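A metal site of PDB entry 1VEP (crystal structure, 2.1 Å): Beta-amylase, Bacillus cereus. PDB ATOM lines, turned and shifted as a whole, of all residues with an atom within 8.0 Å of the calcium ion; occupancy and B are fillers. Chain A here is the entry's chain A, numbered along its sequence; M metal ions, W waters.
The side-chain amino group of Lys 140 lies within salt-bridge range of the side-chain carboxylate of Asp 60. The side-chain carboxylate of Glu 141 is in salt-bridge range of the side-chain amino group of Lys 140 (2.7 Å). The side-chain carboxylate of Glu 141 sits close to the side-chain amide oxygen of Gln 110 (2.8 Å). O of Glu 56 sits at hydrogen-bond distance from NE1 of Trp 106, 3.0 Å away. The side-chain carboxylate (OE1) of Glu 56 sits at hydrogen-bond distance from the indole nitrogen (NE1) of Trp 52 (2.6 Å). OE2 of Glu 144 is in salt-bridge range of NZ of Lys 140, at 3.8 Å.
CH2 of Trp 106 touches the calcium ion, 3.98 Å away. Lys 140 touches the calcium ion (NZ to CA, 3.9 Å). Seven residues have an atom within 4 Å of the calcium ion: Glu 56, Asp 60, Gln 61, Trp 106, Lys 140, Glu 141 and Glu 144. The nearest printed residue that does not touch the calcium ion is Phe 63 (4.5 Å).
The calcium ion is bound by the side-chain carboxylate (OD1) of Asp 60 (2.3 Å). The calcium ion is bound by OE1 of Glu 141. The calcium ion is bound by OE2 of Glu 56, at 2.6 Å. The calcium ion is bound by the side-chain carboxylate (OE1) of Glu 144 (2.6 Å). Water W1 binds the calcium ion (2.7 Å). OE1 of Gln 61 is bound to the calcium ion.
Water W1 lies within hydrogen-bond range of O of Glu 141, OE1 of Glu 56 and N of Leu 145.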
ATOM      1  N   TRP A  52     -28.250  21.994  -9.369  1.00  0.00           N
ATOM      2  CA  TRP A  52     -27.464  23.174  -9.689  1.00  0.00           C
ATOM      3  C   TRP A  52     -26.848  23.674  -8.394  1.00  0.00           C
ATOM      4  O   TRP A  52     -25.688  24.091  -8.367  1.00  0.00           O
ATOM      5  CB  TRP A  52     -28.385  24.245 -10.288  1.00  0.00           C
ATOM      6  CG  TRP A  52     -27.652  25.445 -10.839  1.00  0.00           C
ATOM      7  CD1 TRP A  52     -26.303  25.583 -11.015  1.00  0.00           C
ATOM      8  CD2 TRP A  52     -28.241  26.659 -11.302  1.00  0.00           C
ATOM      9  NE1 TRP A  52     -26.013  26.811 -11.565  1.00  0.00           N
ATOM     10  CE2 TRP A  52     -27.187  27.493 -11.756  1.00  0.00           C
ATOM     11  CE3 TRP A  52     -29.564  27.122 -11.394  1.00  0.00           C
ATOM     12  CZ2 TRP A  52     -27.416  28.767 -12.279  1.00  0.00           C
ATOM     13  CZ3 TRP A  52     -29.792  28.396 -11.917  1.00  0.00           C
ATOM     14  CH2 TRP A  52     -28.720  29.203 -12.356  1.00  0.00           C
ATOM     15  N   GLU A  56     -22.658  24.294  -8.747  1.00  0.00           N
ATOM     16  CA  GLU A  56     -22.117  25.639  -8.889  1.00  0.00           C
ATOM     17  C   GLU A  56     -22.491  26.438  -7.650  1.00  0.00           C
ATOM     18  O   GLU A  56     -22.914  27.587  -7.723  1.00  0.00           O
ATOM     19  CB  GLU A  56     -22.691  26.279 -10.165  1.00  0.00           C
ATOM     20  CG  GLU A  56     -22.142  27.650 -10.495  1.00  0.00           C
ATOM     21  CD  GLU A  56     -22.569  28.138 -11.885  1.00  0.00           C
ATOM     22  OE1 GLU A  56     -23.669  27.754 -12.338  1.00  0.00           O
ATOM     23  OE2 GLU A  56     -21.807  28.909 -12.499  1.00  0.00           O
ATOM     24  N   GLY A  59     -19.812  29.896  -6.425  1.00  0.00           N
ATOM     25  CA  GLY A  59     -19.946  31.122  -7.178  1.00  0.00           C
ATOM     26  C   GLY A  59     -20.050  30.895  -8.662  1.00  0.00           C
ATOM     27  O   GLY A  59     -20.014  29.761  -9.139  1.00  0.00           O
ATOM     28  N   ASP A  60     -20.188  31.986  -9.406  1.00  0.00           N
ATOM     29  CA  ASP A  60     -20.313  31.882 -10.856  1.00  0.00           C
ATOM     30  C   ASP A  60     -19.059  31.238 -11.432  1.00  0.00           C
ATOM     31  O   ASP A  60     -17.942  31.644 -11.119  1.00  0.00           O
ATOM     32  CB  ASP A  60     -20.518  33.265 -11.478  1.00  0.00           C
ATOM     33  CG  ASP A  60     -20.725  33.205 -12.974  1.00  0.00           C
ATOM     34  OD1 ASP A  60     -21.637  32.486 -13.425  1.00  0.00           O
ATOM     35  OD2 ASP A  60     -19.968  33.871 -13.725  1.00  0.00           O
ATOM     36  N   GLN A  61     -19.269  30.229 -12.273  1.00  0.00           N
ATOM     37  CA  GLN A  61     -18.171  29.519 -12.930  1.00  0.00           C
ATOM     38  C   GLN A  61     -17.283  28.692 -11.997  1.00  0.00           C
ATOM     39  O   GLN A  61     -16.215  28.237 -12.409  1.00  0.00           O
ATOM     40  CB  GLN A  61     -17.313  30.500 -13.729  1.00  0.00           C
ATOM     41  CG  GLN A  61     -18.043  31.208 -14.864  1.00  0.00           C
ATOM     42  CD  GLN A  61     -18.736  30.221 -15.793  1.00  0.00           C
ATOM     43  OE1 GLN A  61     -19.804  29.696 -15.483  1.00  0.00           O
ATOM     44  NE2 GLN A  61     -18.130  29.973 -16.955  1.00  0.00           N
ATOM     45  N   GLN A  62     -17.716  28.506 -10.751  1.00  0.00           N
ATOM     46  CA  GLN A  62     -16.961  27.695  -9.788  1.00  0.00           C
ATOM     47  C   GLN A  62     -17.715  26.377  -9.689  1.00  0.00           C
ATOM     48  O   GLN A  62     -18.541  26.161  -8.792  1.00  0.00           O
ATOM     49  CB  GLN A  62     -16.898  28.403  -8.443  1.00  0.00           C
ATOM     50  CG  GLN A  62     -16.161  29.720  -8.517  1.00  0.00           C
ATOM     51  CD  GLN A  62     -16.089  30.444  -7.181  1.00  0.00           C
ATOM     52  OE1 GLN A  62     -15.787  31.636  -7.133  1.00  0.00           O
ATOM     53  NE2 GLN A  62     -16.359  29.732  -6.099  1.00  0.00           N
ATOM     54  N   PHE A  63     -17.419  25.485 -10.640  1.00  0.00           N
ATOM     55  CA  PHE A  63     -18.082  24.199 -10.748  1.00  0.00           C
ATOM     56  C   PHE A  63     -17.495  23.040  -9.958  1.00  0.00           C
ATOM     57  O   PHE A  63     -16.302  23.008  -9.636  1.00  0.00           O
ATOM     58  CB  PHE A  63     -18.163  23.797 -12.223  1.00  0.00           C
ATOM     59  CG  PHE A  63     -18.950  24.748 -13.070  1.00  0.00           C
ATOM     60  CD1 PHE A  63     -20.301  24.980 -12.819  1.00  0.00           C
ATOM     61  CD2 PHE A  63     -18.349  25.408 -14.147  1.00  0.00           C
ATOM     62  CE1 PHE A  63     -21.041  25.848 -13.632  1.00  0.00           C
ATOM     63  CE2 PHE A  63     -19.080  26.267 -14.966  1.00  0.00           C
ATOM     64  CZ  PHE A  63     -20.435  26.497 -14.701  1.00  0.00           C
ATOM     65  N   TRP A 106     -25.919  33.108  -5.113  1.00  0.00           N
ATOM     66  CA  TRP A 106     -25.354  34.244  -5.840  1.00  0.00           C
ATOM     67  C   TRP A 106     -26.125  34.642  -7.095  1.00  0.00           C
ATOM     68  O   TRP A 106     -26.094  35.807  -7.495  1.00  0.00           O
ATOM     69  CB  TRP A 106     -23.900  33.963  -6.205  1.00  0.00           C
ATOM     70  CG  TRP A 106     -23.718  32.683  -6.938  1.00  0.00           C
ATOM     71  CD1 TRP A 106     -23.448  31.460  -6.400  1.00  0.00           C
ATOM     72  CD2 TRP A 106     -23.823  32.484  -8.357  1.00  0.00           C
ATOM     73  NE1 TRP A 106     -23.378  30.509  -7.401  1.00  0.00           N
ATOM     74  CE2 TRP A 106     -23.605  31.112  -8.610  1.00  0.00           C
ATOM     75  CE3 TRP A 106     -24.082  33.334  -9.442  1.00  0.00           C
ATOM     76  CZ2 TRP A 106     -23.644  30.565  -9.899  1.00  0.00           C
ATOM     77  CZ3 TRP A 106     -24.116  32.800 -10.728  1.00  0.00           C
ATOM     78  CH2 TRP A 106     -23.896  31.423 -10.943  1.00  0.00           C
ATOM     79  N   VAL A 107     -26.801  33.693  -7.711  1.00  0.00           N
ATOM     80  CA  VAL A 107     -27.544  33.993  -8.933  1.00  0.00           C
ATOM     81  C   VAL A 107     -28.573  35.113  -8.712  1.00  0.00           C
ATOM     82  O   VAL A 107     -28.884  35.873  -9.628  1.00  0.00           O
ATOM     83  CB  VAL A 107     -28.280  32.745  -9.454  1.00  0.00           C
ATOM     84  CG1 VAL A 107     -29.530  32.468  -8.622  1.00  0.00           C
ATOM     85  CG2 VAL A 107     -28.647  32.927 -10.911  1.00  0.00           C
ATOM     86  N   GLN A 110     -27.629  38.945  -9.422  1.00  0.00           N
ATOM     87  CA  GLN A 110     -27.374  39.410 -10.777  1.00  0.00           C
ATOM     88  C   GLN A 110     -28.353  40.486 -11.250  1.00  0.00           C
ATOM     89  O   GLN A 110     -28.149  41.081 -12.309  1.00  0.00           O
ATOM     90  CB  GLN A 110     -27.388  38.234 -11.736  1.00  0.00           C
ATOM     91  CG  GLN A 110     -26.147  37.386 -11.672  1.00  0.00           C
ATOM     92  CD  GLN A 110     -26.069  36.407 -12.819  1.00  0.00           C
ATOM     93  OE1 GLN A 110     -25.035  35.758 -13.047  1.00  0.00           O
ATOM     94  NE2 GLN A 110     -27.165  36.277 -13.559  1.00  0.00           N
ATOM     95  N   VAL A 137     -30.619  36.130 -18.425  1.00  0.00           N
ATOM     96  CA  VAL A 137     -29.865  35.469 -17.363  1.00  0.00           C
ATOM     97  C   VAL A 137     -29.901  33.964 -17.576  1.00  0.00           C
ATOM     98  O   VAL A 137     -28.898  33.283 -17.414  1.00  0.00           O
ATOM     99  CB  VAL A 137     -30.463  35.799 -15.970  1.00  0.00           C
ATOM    100  CG1 VAL A 137     -29.843  34.898 -14.915  1.00  0.00           C
ATOM    101  CG2 VAL A 137     -30.189  37.248 -15.630  1.00  0.00           C
ATOM    102  N   LYS A 140     -27.412  32.871 -20.226  1.00  0.00           N
ATOM    103  CA  LYS A 140     -26.047  32.862 -19.728  1.00  0.00           C
ATOM    104  C   LYS A 140     -25.740  31.694 -18.783  1.00  0.00           C
ATOM    105  O   LYS A 140     -24.810  30.924 -19.030  1.00  0.00           O
ATOM    106  CB  LYS A 140     -25.732  34.164 -18.991  1.00  0.00           C
ATOM    107  CG  LYS A 140     -24.374  34.130 -18.305  1.00  0.00           C
ATOM    108  CD  LYS A 140     -24.144  35.356 -17.428  1.00  0.00           C
ATOM    109  CE  LYS A 140     -22.760  35.329 -16.793  1.00  0.00           C
ATOM    110  NZ  LYS A 140     -22.603  34.228 -15.789  1.00  0.00           N
ATOM    111  N   GLU A 141     -26.515  31.584 -17.707  1.00  0.00           N
ATOM    112  CA  GLU A 141     -26.287  30.545 -16.707  1.00  0.00           C
ATOM    113  C   GLU A 141     -26.511  29.100 -17.168  1.00  0.00           C
ATOM    114  O   GLU A 141     -25.663  28.238 -16.953  1.00  0.00           O
ATOM    115  CB  GLU A 141     -27.155  30.817 -15.468  1.00  0.00           C
ATOM    116  CG  GLU A 141     -26.914  32.168 -14.804  1.00  0.00           C
ATOM    117  CD  GLU A 141     -25.447  32.467 -14.581  1.00  0.00           C
ATOM    118  OE1 GLU A 141     -24.702  31.556 -14.137  1.00  0.00           O
ATOM    119  OE2 GLU A 141     -25.035  33.607 -14.841  1.00  0.00           O
ATOM    120  N   TYR A 142     -27.653  28.822 -17.785  1.00  0.00           N
ATOM    121  CA  TYR A 142     -27.926  27.467 -18.249  1.00  0.00           C
ATOM    122  C   TYR A 142     -26.913  27.132 -19.308  1.00  0.00           C
ATOM    123  O   TYR A 142     -26.402  26.023 -19.365  1.00  0.00           O
ATOM    124  CB  TYR A 142     -29.343  27.345 -18.820  1.00  0.00           C
ATOM    125  CG  TYR A 142     -30.455  27.336 -17.779  1.00  0.00           C
ATOM    126  CD1 TYR A 142     -30.349  28.064 -16.598  1.00  0.00           C
ATOM    127  CD2 TYR A 142     -31.642  26.645 -18.028  1.00  0.00           C
ATOM    128  CE1 TYR A 142     -31.407  28.121 -15.678  1.00  0.00           C
ATOM    129  CE2 TYR A 142     -32.709  26.701 -17.119  1.00  0.00           C
ATOM    130  CZ  TYR A 142     -32.586  27.436 -15.953  1.00  0.00           C
ATOM    131  OH  TYR A 142     -33.650  27.528 -15.088  1.00  0.00           O
ATOM    132  N   GLY A 143     -26.621  28.120 -20.146  1.00  0.00           N
ATOM    133  CA  GLY A 143     -25.653  27.932 -21.218  1.00  0.00           C
ATOM    134  C   GLY A 143     -24.296  27.488 -20.676  1.00  0.00           C
ATOM    135  O   GLY A 143     -23.707  26.536 -21.197  1.00  0.00           O
ATOM    136  N   GLU A 144     -23.819  28.158 -19.636  1.00  0.00           N
ATOM    137  CA  GLU A 144     -22.526  27.822 -19.038  1.00  0.00           C
ATOM    138  C   GLU A 144     -22.579  26.508 -18.262  1.00  0.00           C
ATOM    139  O   GLU A 144     -21.657  25.703 -18.337  1.00  0.00           O
ATOM    140  CB  GLU A 144     -22.058  28.970 -18.136  1.00  0.00           C
ATOM    141  CG  GLU A 144     -21.901  30.283 -18.882  1.00  0.00           C
ATOM    142  CD  GLU A 144     -21.571  31.448 -17.973  1.00  0.00           C
ATOM    143  OE1 GLU A 144     -22.204  31.582 -16.917  1.00  0.00           O
ATOM    144  OE2 GLU A 144     -20.675  32.246 -18.331  1.00  0.00           O
ATOM    145  N   LEU A 145     -23.671  26.296 -17.519  1.00  0.00           N
ATOM    146  CA  LEU A 145     -23.837  25.080 -16.749  1.00  0.00           C
ATOM    147  C   LEU A 145     -23.823  23.872 -17.691  1.00  0.00           C
ATOM    148  O   LEU A 145     -23.043  22.942 -17.504  1.00  0.00           O
ATOM    149  CB  LEU A 145     -25.155  25.109 -15.965  1.00  0.00           C
ATOM    150  CG  LEU A 145     -25.478  23.871 -15.119  1.00  0.00           C
ATOM    151  CD1 LEU A 145     -24.431  23.708 -14.011  1.00  0.00           C
ATOM    152  CD2 LEU A 145     -26.884  23.967 -14.521  1.00  0.00           C
ATOM    153  N   ALA A 148     -20.425  23.223 -19.234  1.00  0.00           N
ATOM    154  CA  ALA A 148     -19.459  22.754 -18.257  1.00  0.00           C
ATOM    155  C   ALA A 148     -19.766  21.287 -17.949  1.00  0.00           C
ATOM    156  O   ALA A 148     -18.863  20.462 -17.816  1.00  0.00           O
ATOM    157  CB  ALA A 148     -19.546  23.594 -16.983  1.00  0.00           C
HETATM  158 CA    CA M   1     -22.317  30.557 -14.490  1.00  0.00          CA
HETATM  159  O   HOH W   1     -23.700  28.390 -15.182  1.00  0.00           O
